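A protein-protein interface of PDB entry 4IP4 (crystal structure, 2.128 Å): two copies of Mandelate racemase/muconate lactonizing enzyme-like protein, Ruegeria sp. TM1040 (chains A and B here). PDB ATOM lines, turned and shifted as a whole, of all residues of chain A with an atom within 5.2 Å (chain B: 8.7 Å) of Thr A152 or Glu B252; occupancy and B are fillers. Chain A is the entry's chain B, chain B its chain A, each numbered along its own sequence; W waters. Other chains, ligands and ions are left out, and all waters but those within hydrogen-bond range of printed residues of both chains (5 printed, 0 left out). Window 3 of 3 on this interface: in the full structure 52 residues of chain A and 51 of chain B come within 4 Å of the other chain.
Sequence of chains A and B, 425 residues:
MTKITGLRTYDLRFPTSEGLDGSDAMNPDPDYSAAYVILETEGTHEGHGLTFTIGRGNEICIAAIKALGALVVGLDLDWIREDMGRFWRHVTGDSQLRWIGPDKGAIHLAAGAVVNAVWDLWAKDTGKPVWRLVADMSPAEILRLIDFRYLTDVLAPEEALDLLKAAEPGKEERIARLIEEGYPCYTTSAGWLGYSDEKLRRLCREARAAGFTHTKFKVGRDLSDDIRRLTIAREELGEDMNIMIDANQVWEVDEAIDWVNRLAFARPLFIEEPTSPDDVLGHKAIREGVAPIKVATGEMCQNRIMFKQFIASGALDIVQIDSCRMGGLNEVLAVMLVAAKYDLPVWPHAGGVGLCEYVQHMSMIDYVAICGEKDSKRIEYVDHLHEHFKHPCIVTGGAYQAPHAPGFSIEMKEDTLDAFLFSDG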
ATOM      1  N   PHE A 148       3.644 -13.672   6.274  1.00  0.00           N
ATOM      2  CA  PHE A 148       2.196 -13.522   6.259  1.00  0.00           C
ATOM      3  C   PHE A 148       1.435 -14.681   5.616  1.00  0.00           C
ATOM      4  O   PHE A 148       0.215 -14.588   5.457  1.00  0.00           O
ATOM      5  CB  PHE A 148       1.811 -12.228   5.541  1.00  0.00           C
ATOM      6  CG  PHE A 148       1.876 -11.013   6.412  1.00  0.00           C
ATOM      7  CD1 PHE A 148       0.772 -10.611   7.144  1.00  0.00           C
ATOM      8  CD2 PHE A 148       3.045 -10.259   6.489  1.00  0.00           C
ATOM      9  CE1 PHE A 148       0.826  -9.478   7.946  1.00  0.00           C
ATOM     10  CE2 PHE A 148       3.108  -9.126   7.285  1.00  0.00           C
ATOM     11  CZ  PHE A 148       1.996  -8.737   8.017  1.00  0.00           C
ATOM     12  N   ARG A 149       2.132 -15.757   5.242  1.00  0.00           N
ATOM     13  CA  ARG A 149       1.460 -16.873   4.573  1.00  0.00           C
ATOM     14  C   ARG A 149       0.349 -17.442   5.442  1.00  0.00           C
ATOM     15  O   ARG A 149       0.553 -17.710   6.631  1.00  0.00           O
ATOM     16  CB  ARG A 149       2.430 -17.990   4.150  1.00  0.00           C
ATOM     17  CG  ARG A 149       1.693 -19.141   3.434  1.00  0.00           C
ATOM     18  CD  ARG A 149       2.622 -20.046   2.628  1.00  0.00           C
ATOM     19  NE  ARG A 149       3.627 -20.662   3.489  1.00  0.00           N
ATOM     20  CZ  ARG A 149       4.419 -21.663   3.117  1.00  0.00           C
ATOM     21  NH1 ARG A 149       4.314 -22.181   1.887  1.00  0.00           N
ATOM     22  NH2 ARG A 149       5.308 -22.150   3.979  1.00  0.00           N
ATOM     23  N   TYR A 150      -0.820 -17.596   4.826  1.00  0.00           N
ATOM     24  CA  TYR A 150      -2.036 -18.086   5.463  1.00  0.00           C
ATOM     25  C   TYR A 150      -2.632 -17.087   6.444  1.00  0.00           C
ATOM     26  O   TYR A 150      -3.477 -17.455   7.261  1.00  0.00           O
ATOM     27  CB  TYR A 150      -1.810 -19.426   6.164  1.00  0.00           C
ATOM     28  CG  TYR A 150      -1.217 -20.511   5.292  1.00  0.00           C
ATOM     29  CD1 TYR A 150      -1.692 -20.742   4.002  1.00  0.00           C
ATOM     30  CD2 TYR A 150      -0.197 -21.322   5.775  1.00  0.00           C
ATOM     31  CE1 TYR A 150      -1.149 -21.755   3.215  1.00  0.00           C
ATOM     32  CE2 TYR A 150       0.349 -22.327   5.002  1.00  0.00           C
ATOM     33  CZ  TYR A 150      -0.129 -22.538   3.726  1.00  0.00           C
ATOM     34  OH  TYR A 150       0.421 -23.543   2.977  1.00  0.00           O
ATOM     35  N   LEU A 151      -2.200 -15.830   6.360  1.00  0.00           N
ATOM     36  CA  LEU A 151      -2.777 -14.766   7.183  1.00  0.00           C
ATOM     37  C   LEU A 151      -3.577 -13.761   6.365  1.00  0.00           C
ATOM     38  O   LEU A 151      -4.396 -13.033   6.922  1.00  0.00           O
ATOM     39  CB  LEU A 151      -1.681 -13.993   7.936  1.00  0.00           C
ATOM     40  CG  LEU A 151      -1.396 -14.362   9.390  1.00  0.00           C
ATOM     41  CD1 LEU A 151      -0.474 -13.317  10.024  1.00  0.00           C
ATOM     42  CD2 LEU A 151      -2.686 -14.520  10.205  1.00  0.00           C
ATOM     43  N   THR A 152      -3.336 -13.724   5.053  1.00  0.00           N
ATOM     44  CA  THR A 152      -3.723 -12.565   4.241  1.00  0.00           C
ATOM     45  C   THR A 152      -5.223 -12.346   4.092  1.00  0.00           C
ATOM     46  O   THR A 152      -5.645 -11.249   3.734  1.00  0.00           O
ATOM     47  CB  THR A 152      -3.075 -12.571   2.833  1.00  0.00           C
ATOM     48  OG1 THR A 152      -3.594 -13.662   2.054  1.00  0.00           O
ATOM     49  CG2 THR A 152      -1.563 -12.675   2.931  1.00  0.00           C
ATOM     50  N   ASP A 153      -6.032 -13.364   4.371  1.00  0.00           N
ATOM     51  CA  ASP A 153      -7.484 -13.172   4.295  1.00  0.00           C
ATOM     52  C   ASP A 153      -8.010 -12.420   5.517  1.00  0.00           C
ATOM     53  O   ASP A 153      -9.107 -11.884   5.487  1.00  0.00           O
ATOM     54  CB  ASP A 153      -8.233 -14.503   4.112  1.00  0.00           C
ATOM     55  CG  ASP A 153      -8.038 -15.454   5.283  1.00  0.00           C
ATOM     56  OD1 ASP A 153      -6.973 -15.394   5.940  1.00  0.00           O
ATOM     57  OD2 ASP A 153      -8.949 -16.267   5.548  1.00  0.00           O
ATOM     58  N   VAL A 154      -7.221 -12.381   6.587  1.00  0.00           N
ATOM     59  CA  VAL A 154      -7.631 -11.700   7.817  1.00  0.00           C
ATOM     60  C   VAL A 154      -6.777 -10.453   8.082  1.00  0.00           C
ATOM     61  O   VAL A 154      -7.280  -9.406   8.493  1.00  0.00           O
ATOM     62  CB  VAL A 154      -7.570 -12.661   9.033  1.00  0.00           C
ATOM     63  CG1 VAL A 154      -7.855 -11.921  10.338  1.00  0.00           C
ATOM     64  CG2 VAL A 154      -8.555 -13.804   8.845  1.00  0.00           C
ATOM     65  N   LEU A 155      -5.480 -10.573   7.837  1.00  0.00           N
ATOM     66  CA  LEU A 155      -4.577  -9.439   7.982  1.00  0.00           C
ATOM     67  C   LEU A 155      -3.526  -9.495   6.894  1.00  0.00           C
ATOM     68  O   LEU A 155      -2.606 -10.311   6.958  1.00  0.00           O
ATOM     69  CB  LEU A 155      -3.899  -9.455   9.351  1.00  0.00           C
ATOM     70  CG  LEU A 155      -2.960  -8.270   9.592  1.00  0.00           C
ATOM     71  CD1 LEU A 155      -3.762  -6.972   9.725  1.00  0.00           C
ATOM     72  CD2 LEU A 155      -2.091  -8.523  10.806  1.00  0.00           C
ATOM     73  N   ALA A 156      -3.676  -8.644   5.886  1.00  0.00           N
ATOM     74  CA  ALA A 156      -2.704  -8.570   4.800  1.00  0.00           C
ATOM     75  C   ALA A 156      -1.609  -7.566   5.181  1.00  0.00           C
ATOM     76  O   ALA A 156      -1.816  -6.734   6.068  1.00  0.00           O
ATOM     77  CB  ALA A 156      -3.405  -8.173   3.489  1.00  0.00           C
ATOM     78  N   PRO A 157      -0.432  -7.655   4.539  1.00  0.00           N
ATOM     79  CA  PRO A 157       0.688  -6.778   4.914  1.00  0.00           C
ATOM     80  C   PRO A 157       0.353  -5.283   4.922  1.00  0.00           C
ATOM     81  O   PRO A 157       0.836  -4.537   5.776  1.00  0.00           O
ATOM     82  CB  PRO A 157       1.728  -7.082   3.837  1.00  0.00           C
ATOM     83  CG  PRO A 157       1.466  -8.516   3.493  1.00  0.00           C
ATOM     84  CD  PRO A 157      -0.026  -8.659   3.538  1.00  0.00           C
ATOM     85  N   GLN B 249      -2.008 -27.373  -0.245  1.00  0.00           N
ATOM     86  CA  GLN B 249      -1.998 -26.286   0.755  1.00  0.00           C
ATOM     87  C   GLN B 249      -1.337 -24.972   0.335  1.00  0.00           C
ATOM     88  O   GLN B 249      -1.256 -24.053   1.150  1.00  0.00           O
ATOM     89  CB  GLN B 249      -1.372 -26.733   2.096  1.00  0.00           C
ATOM     90  CG  GLN B 249      -1.835 -28.094   2.623  1.00  0.00           C
ATOM     91  CD  GLN B 249      -0.872 -28.666   3.653  1.00  0.00           C
ATOM     92  OE1 GLN B 249       0.175 -28.078   3.932  1.00  0.00           O
ATOM     93  NE2 GLN B 249      -1.217 -29.821   4.215  1.00  0.00           N
ATOM     94  N   VAL B 250      -0.869 -24.860  -0.905  1.00  0.00           N
ATOM     95  CA  VAL B 250       0.080 -23.777  -1.226  1.00  0.00           C
ATOM     96  C   VAL B 250      -0.474 -22.358  -1.326  1.00  0.00           C
ATOM     97  O   VAL B 250       0.300 -21.405  -1.291  1.00  0.00           O
ATOM     98  CB  VAL B 250       0.905 -24.052  -2.510  1.00  0.00           C
ATOM     99  CG1 VAL B 250       1.808 -25.267  -2.324  1.00  0.00           C
ATOM    100  CG2 VAL B 250      -0.011 -24.229  -3.721  1.00  0.00           C
ATOM    101  N   TRP B 251      -1.791 -22.210  -1.468  1.00  0.00           N
ATOM    102  CA  TRP B 251      -2.380 -20.899  -1.789  1.00  0.00           C
ATOM    103  C   TRP B 251      -2.941 -20.137  -0.586  1.00  0.00           C
ATOM    104  O   TRP B 251      -3.353 -20.742   0.408  1.00  0.00           O
ATOM    105  CB  TRP B 251      -3.536 -21.062  -2.772  1.00  0.00           C
ATOM    106  CG  TRP B 251      -3.196 -21.626  -4.122  1.00  0.00           C
ATOM    107  CD1 TRP B 251      -2.113 -21.328  -4.898  1.00  0.00           C
ATOM    108  CD2 TRP B 251      -3.970 -22.582  -4.858  1.00  0.00           C
ATOM    109  NE1 TRP B 251      -2.171 -22.039  -6.081  1.00  0.00           N
ATOM    110  CE2 TRP B 251      -3.299 -22.820  -6.074  1.00  0.00           C
ATOM    111  CE3 TRP B 251      -5.164 -23.264  -4.601  1.00  0.00           C
ATOM    112  CZ2 TRP B 251      -3.787 -23.702  -7.033  1.00  0.00           C
ATOM    113  CZ3 TRP B 251      -5.647 -24.143  -5.554  1.00  0.00           C
ATOM    114  CH2 TRP B 251      -4.959 -24.354  -6.755  1.00  0.00           C
ATOM    115  N   GLU B 252      -2.981 -18.810  -0.712  1.00  0.00           N
ATOM    116  CA  GLU B 252      -3.833 -17.951   0.112  1.00  0.00           C
ATOM    117  C   GLU B 252      -5.276 -18.161  -0.350  1.00  0.00           C
ATOM    118  O   GLU B 252      -5.513 -18.687  -1.434  1.00  0.00           O
ATOM    119  CB  GLU B 252      -3.467 -16.467  -0.081  1.00  0.00           C
ATOM    120  CG  GLU B 252      -2.062 -16.087   0.393  1.00  0.00           C
ATOM    121  CD  GLU B 252      -1.849 -16.435   1.864  1.00  0.00           C
ATOM    122  OE1 GLU B 252      -0.942 -17.241   2.163  1.00  0.00           O
ATOM    123  OE2 GLU B 252      -2.605 -15.905   2.714  1.00  0.00           O
ATOM    124  N   VAL B 253      -6.230 -17.711   0.457  1.00  0.00           N
ATOM    125  CA  VAL B 253      -7.649 -17.848   0.135  1.00  0.00           C
ATOM    126  C   VAL B 253      -8.008 -17.173  -1.189  1.00  0.00           C
ATOM    127  O   VAL B 253      -8.619 -17.804  -2.059  1.00  0.00           O
ATOM    128  CB  VAL B 253      -8.531 -17.283   1.272  1.00  0.00           C
ATOM    129  CG1 VAL B 253      -9.962 -17.135   0.826  1.00  0.00           C
ATOM    130  CG2 VAL B 253      -8.436 -18.171   2.509  1.00  0.00           C
ATOM    131  N   ASP B 254      -7.620 -15.907  -1.355  1.00  0.00           N
ATOM    132  CA  ASP B 254      -7.984 -15.171  -2.571  1.00  0.00           C
ATOM    133  C   ASP B 254      -7.305 -15.748  -3.809  1.00  0.00           C
ATOM    134  O   ASP B 254      -7.920 -15.877  -4.871  1.00  0.00           O
ATOM    135  CB  ASP B 254      -7.729 -13.658  -2.434  1.00  0.00           C
ATOM    136  CG  ASP B 254      -6.254 -13.303  -2.249  1.00  0.00           C
ATOM    137  OD1 ASP B 254      -5.409 -14.200  -2.037  1.00  0.00           O
ATOM    138  OD2 ASP B 254      -5.939 -12.093  -2.303  1.00  0.00           O
ATOM    139  N   GLU B 255      -6.039 -16.102  -3.643  1.00  0.00           N
ATOM    140  CA  GLU B 255      -5.240 -16.767  -4.667  1.00  0.00           C
ATOM    141  C   GLU B 255      -5.830 -18.118  -5.098  1.00  0.00           C
ATOM    142  O   GLU B 255      -5.841 -18.463  -6.292  1.00  0.00           O
ATOM    143  CB  GLU B 255      -3.835 -16.988  -4.113  1.00  0.00           C
ATOM    144  CG  GLU B 255      -2.897 -17.737  -5.032  1.00  0.00           C
ATOM    145  CD  GLU B 255      -1.527 -17.947  -4.399  1.00  0.00           C
ATOM    146  OE1 GLU B 255      -1.421 -17.893  -3.143  1.00  0.00           O
ATOM    147  OE2 GLU B 255      -0.559 -18.149  -5.163  1.00  0.00           O
ATOM    148  N   ALA B 256      -6.296 -18.895  -4.126  1.00  0.00           N
ATOM    149  CA  ALA B 256      -6.897 -20.195  -4.426  1.00  0.00           C
ATOM    150  C   ALA B 256      -8.143 -20.047  -5.292  1.00  0.00           C
ATOM    151  O   ALA B 256      -8.352 -20.807  -6.239  1.00  0.00           O
ATOM    152  CB  ALA B 256      -7.244 -20.948  -3.136  1.00  0.00           C
ATOM    153  N   ILE B 257      -8.972 -19.068  -4.960  1.00  0.00           N
ATOM    154  CA  ILE B 257     -10.215 -18.864  -5.688  1.00  0.00           C
ATOM    155  C   ILE B 257      -9.939 -18.509  -7.149  1.00  0.00           C
ATOM    156  O   ILE B 257     -10.546 -19.073  -8.066  1.00  0.00           O
ATOM    157  CB  ILE B 257     -11.096 -17.786  -5.007  1.00  0.00           C
ATOM    158  CG1 ILE B 257     -11.508 -18.243  -3.595  1.00  0.00           C
ATOM    159  CG2 ILE B 257     -12.316 -17.466  -5.866  1.00  0.00           C
ATOM    160  CD1 ILE B 257     -12.187 -17.142  -2.766  1.00  0.00           C
ATOM    161  N   ASP B 258      -9.011 -17.587  -7.374  1.00  0.00           N
ATOM    162  CA  ASP B 258      -8.668 -17.190  -8.740  1.00  0.00           C
ATOM    163  C   ASP B 258      -8.034 -18.316  -9.559  1.00  0.00           C
ATOM    164  O   ASP B 258      -8.331 -18.487 -10.738  1.00  0.00           O
ATOM    165  CB  ASP B 258      -7.722 -16.009  -8.706  1.00  0.00           C
ATOM    166  CG  ASP B 258      -8.371 -14.769  -8.131  1.00  0.00           C
ATOM    167  OD1 ASP B 258      -9.625 -14.695  -8.072  1.00  0.00           O
ATOM    168  OD2 ASP B 258      -7.615 -13.864  -7.746  1.00  0.00           O
ATOM    169  N   TRP B 259      -7.142 -19.065  -8.927  1.00  0.00           N
ATOM    170  CA  TRP B 259      -6.380 -20.098  -9.611  1.00  0.00           C
ATOM    171  C   TRP B 259      -7.271 -21.292  -9.982  1.00  0.00           C
ATOM    172  O   TRP B 259      -7.233 -21.759 -11.121  1.00  0.00           O
ATOM    173  CB  TRP B 259      -5.208 -20.522  -8.734  1.00  0.00           C
ATOM    174  CG  TRP B 259      -4.150 -21.366  -9.373  1.00  0.00           C
ATOM    175  CD1 TRP B 259      -4.322 -22.531 -10.075  1.00  0.00           C
ATOM    176  CD2 TRP B 259      -2.737 -21.145  -9.298  1.00  0.00           C
ATOM    177  NE1 TRP B 259      -3.096 -23.033 -10.461  1.00  0.00           N
ATOM    178  CE2 TRP B 259      -2.110 -22.201  -9.991  1.00  0.00           C
ATOM    179  CE3 TRP B 259      -1.941 -20.152  -8.714  1.00  0.00           C
ATOM    180  CZ2 TRP B 259      -0.723 -22.287 -10.119  1.00  0.00           C
ATOM    181  CZ3 TRP B 259      -0.560 -20.237  -8.845  1.00  0.00           C
ATOM    182  CH2 TRP B 259       0.032 -21.300  -9.538  1.00  0.00           C
ATOM    183  N   VAL B 260      -8.083 -21.794  -9.053  1.00  0.00           N
ATOM    184  CA  VAL B 260      -8.948 -22.895  -9.450  1.00  0.00           C
ATOM    185  C   VAL B 260     -10.069 -22.457 -10.396  1.00  0.00           C
ATOM    186  O   VAL B 260     -10.455 -23.211 -11.282  1.00  0.00           O
ATOM    187  CB  VAL B 260      -9.468 -23.830  -8.292  1.00  0.00           C
ATOM    188  CG1 VAL B 260      -8.736 -23.622  -6.993  1.00  0.00           C
ATOM    189  CG2 VAL B 260     -10.976 -23.763  -8.137  1.00  0.00           C
ATOM    190  N   GLU B 273      -7.162 -29.532  -0.654  1.00  0.00           N
ATOM    191  CA  GLU B 273      -6.215 -28.694   0.098  1.00  0.00           C
ATOM    192  C   GLU B 273      -5.814 -27.394  -0.614  1.00  0.00           C
ATOM    193  O   GLU B 273      -4.626 -27.161  -0.874  1.00  0.00           O
ATOM    194  CB  GLU B 273      -4.963 -29.492   0.433  1.00  0.00           C
ATOM    195  CG  GLU B 273      -5.213 -30.641   1.386  1.00  0.00           C
ATOM    196  CD  GLU B 273      -3.998 -30.905   2.247  1.00  0.00           C
ATOM    197  OE1 GLU B 273      -3.018 -31.487   1.723  1.00  0.00           O
ATOM    198  OE2 GLU B 273      -4.014 -30.501   3.438  1.00  0.00           O
ATOM    199  N   PRO B 274      -6.801 -26.542  -0.937  1.00  0.00           N
ATOM    200  CA  PRO B 274      -6.433 -25.292  -1.603  1.00  0.00           C
ATOM    201  C   PRO B 274      -5.600 -24.403  -0.672  1.00  0.00           C
ATOM    202  O   PRO B 274      -4.866 -23.546  -1.152  1.00  0.00           O
ATOM    203  CB  PRO B 274      -7.783 -24.638  -1.890  1.00  0.00           C
ATOM    204  CG  PRO B 274      -8.696 -25.196  -0.826  1.00  0.00           C
ATOM    205  CD  PRO B 274      -8.245 -26.613  -0.648  1.00  0.00           C
ATOM    206  N   THR B 275      -5.710 -24.607   0.637  1.00  0.00           N
ATOM    207  CA  THR B 275      -4.924 -23.808   1.570  1.00  0.00           C
ATOM    208  C   THR B 275      -4.533 -24.589   2.832  1.00  0.00           C
ATOM    209  O   THR B 275      -4.697 -25.810   2.883  1.00  0.00           O
ATOM    210  CB  THR B 275      -5.630 -22.477   1.915  1.00  0.00           C
ATOM    211  OG1 THR B 275      -4.699 -21.598   2.557  1.00  0.00           O
ATOM    212  CG2 THR B 275      -6.836 -22.703   2.814  1.00  0.00           C
ATOM    213  N   SER B 276      -3.990 -23.885   3.824  1.00  0.00           N
ATOM    214  CA  SER B 276      -3.506 -24.504   5.059  1.00  0.00           C
ATOM    215  C   SER B 276      -4.498 -25.487   5.665  1.00  0.00           C
ATOM    216  O   SER B 276      -5.695 -25.217   5.708  1.00  0.00           O
ATOM    217  CB  SER B 276      -3.178 -23.431   6.099  1.00  0.00           C
ATOM    218  OG  SER B 276      -2.962 -24.030   7.370  1.00  0.00           O
ATOM    219  N   ASP B 279      -6.995 -24.181   8.338  1.00  0.00           N
ATOM    220  CA  ASP B 279      -7.839 -23.019   8.083  1.00  0.00           C
ATOM    221  C   ASP B 279      -9.269 -23.438   7.727  1.00  0.00           C
ATOM    222  O   ASP B 279      -9.613 -23.610   6.558  1.00  0.00           O
ATOM    223  CB  ASP B 279      -7.227 -22.146   6.982  1.00  0.00           C
ATOM    224  CG  ASP B 279      -7.760 -20.722   6.992  1.00  0.00           C
ATOM    225  OD1 ASP B 279      -8.723 -20.431   7.743  1.00  0.00           O
ATOM    226  OD2 ASP B 279      -7.209 -19.890   6.237  1.00  0.00           O
ATOM    227  N   GLY B 282     -11.065 -20.338   6.219  1.00  0.00           N
ATOM    228  CA  GLY B 282     -10.504 -20.138   4.891  1.00  0.00           C
ATOM    229  C   GLY B 282     -11.011 -21.140   3.858  1.00  0.00           C
ATOM    230  O   GLY B 282     -11.364 -20.759   2.743  1.00  0.00           O
ATOM    231  N   HIS B 283     -11.049 -22.424   4.212  1.00  0.00           N
ATOM    232  CA  HIS B 283     -11.641 -23.416   3.309  1.00  0.00           C
ATOM    233  C   HIS B 283     -13.099 -23.067   2.987  1.00  0.00           C
ATOM    234  O   HIS B 283     -13.540 -23.169   1.839  1.00  0.00           O
ATOM    235  CB  HIS B 283     -11.523 -24.835   3.877  1.00  0.00           C
ATOM    236  CG  HIS B 283     -10.203 -25.484   3.597  1.00  0.00           C
ATOM    237  ND1 HIS B 283      -9.095 -25.301   4.399  1.00  0.00           N
ATOM    238  CD2 HIS B 283      -9.804 -26.293   2.584  1.00  0.00           C
ATOM    239  CE1 HIS B 283      -8.076 -25.984   3.903  1.00  0.00           C
ATOM    240  NE2 HIS B 283      -8.478 -26.593   2.800  1.00  0.00           N
ATOM    241  N   ILE B 286     -13.111 -20.278   0.477  1.00  0.00           N
ATOM    242  CA  ILE B 286     -12.699 -20.794  -0.837  1.00  0.00           C
ATOM    243  C   ILE B 286     -13.846 -21.578  -1.486  1.00  0.00           C
ATOM    244  O   ILE B 286     -14.149 -21.406  -2.671  1.00  0.00           O
ATOM    245  CB  ILE B 286     -11.440 -21.670  -0.734  1.00  0.00           C
ATOM    246  CG1 ILE B 286     -10.247 -20.834  -0.253  1.00  0.00           C
ATOM    247  CG2 ILE B 286     -11.122 -22.336  -2.091  1.00  0.00           C
ATOM    248  CD1 ILE B 286      -9.056 -21.689   0.198  1.00  0.00           C
HETATM  249  O   HOH W   1      -6.532 -14.241   0.975  1.00  0.00           O
HETATM  250  O   HOH W   2      -3.542 -12.883  -0.416  1.00  0.00           O
HETATM  251  O   HOH W   3      -9.690 -17.955   7.755  1.00  0.00           O
HETATM  252  O   HOH W   4       2.702 -21.582  -0.516  1.00  0.00           O
HETATM  253  O   HOH W   5       0.558 -25.559   4.872  1.00  0.00           O
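Water W4 lies within hydrogen-bond range of the backbone carbonyl oxygen of Val B250 (2.5 Å) and the guanidinium group of Arg A149 (3.0 Å).
Water W2 bridges the side-chain hydroxyl (OG1) of Thr A152 (2.6 Å) and the side-chain carboxylate (OD1) of Asp B254 (2.8 Å).
Water W3 lies within hydrogen-bond range of OD1 of Asp B279 (2.7 Å), OD2 of Asp A153 (2.9 Å) and N of Gly B282 (3.2 Å).
Water W5 bridges OE1 of Gln B249 and OH of Tyr A150.
Water W1 lies within hydrogen-bond range of N of Asp B254 (3.1 Å) and OG1 of Thr A152 (3.2 Å).
Thr A152 touches just one residue of chain B: Glu B252.
Of the printed residues of chain B, Leu A151 touches Glu B252 (3.7 Å).
Printed residues of chain A within 4 Å of Val B253: Asp A153 (3.6 Å).
Of the printed residues of chain A, Trp B251 touches Tyr A150 (3.7 Å).
Of the printed residues of chain A, Ser B276 touches Tyr A150 (3.6 Å).
Of the printed residues of chain B, Arg A149 touches Glu B252 (3.4 Å).
The nearest printed residue of chain A that does not touch Val B253 is Thr A152 (5.1 Å).
The side-chain hydroxyl of Tyr A150 is in hydrogen-bond range of the backbone carbonyl oxygen of Gln B249 (2.5 Å).
OE1 of Glu B252 is in hydrogen-bond range of N of Tyr A150.
The side-chain carboxylate of Glu B252 is in hydrogen-bond range of the side-chain hydroxyl of Thr A152, at 2.5 Å.
Printed residues of chain B that touch a printed residue of chain A: Gln B249, Trp B251, Glu B252, Val B253, Thr B275 and Ser B276.
Hydrophobic or aromatic side chains of chain B that line the printed part of chain A: Val B253.
Among the printed residues, no Asp or Glu carboxylate lies within 4 Å of a Lys or Arg side-chain nitrogen of the other chain.
No position is printed for both chains.
Among the printed residues, pairs that only touch across the chains: Arg A149 with Glu B252, Tyr A150 with Trp B251, Tyr A150 with Thr B275, Tyr A150 with Ser B276, Leu A151 with Glu B252 and Asp A153 with Val B253.
The backbone NH (N) of Gln B249 sits at hydrogen-bond distance from the backbone carbonyl oxygen (O) of Glu B273 (2.7 Å).
The backbone NH of Trp B251 lies close to the backbone carbonyl oxygen of Pro B274, at 3.4 Å.
The backbone carbonyl oxygen (O) of Trp B251 is in hydrogen-bond range of the side-chain hydroxyl (OG1) of Thr B275, at 2.7 Å.
The backbone NH (N) of Glu B252 sits at hydrogen-bond distance from the side-chain carboxylate (OE1) of Glu B255, at 3.0 Å.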
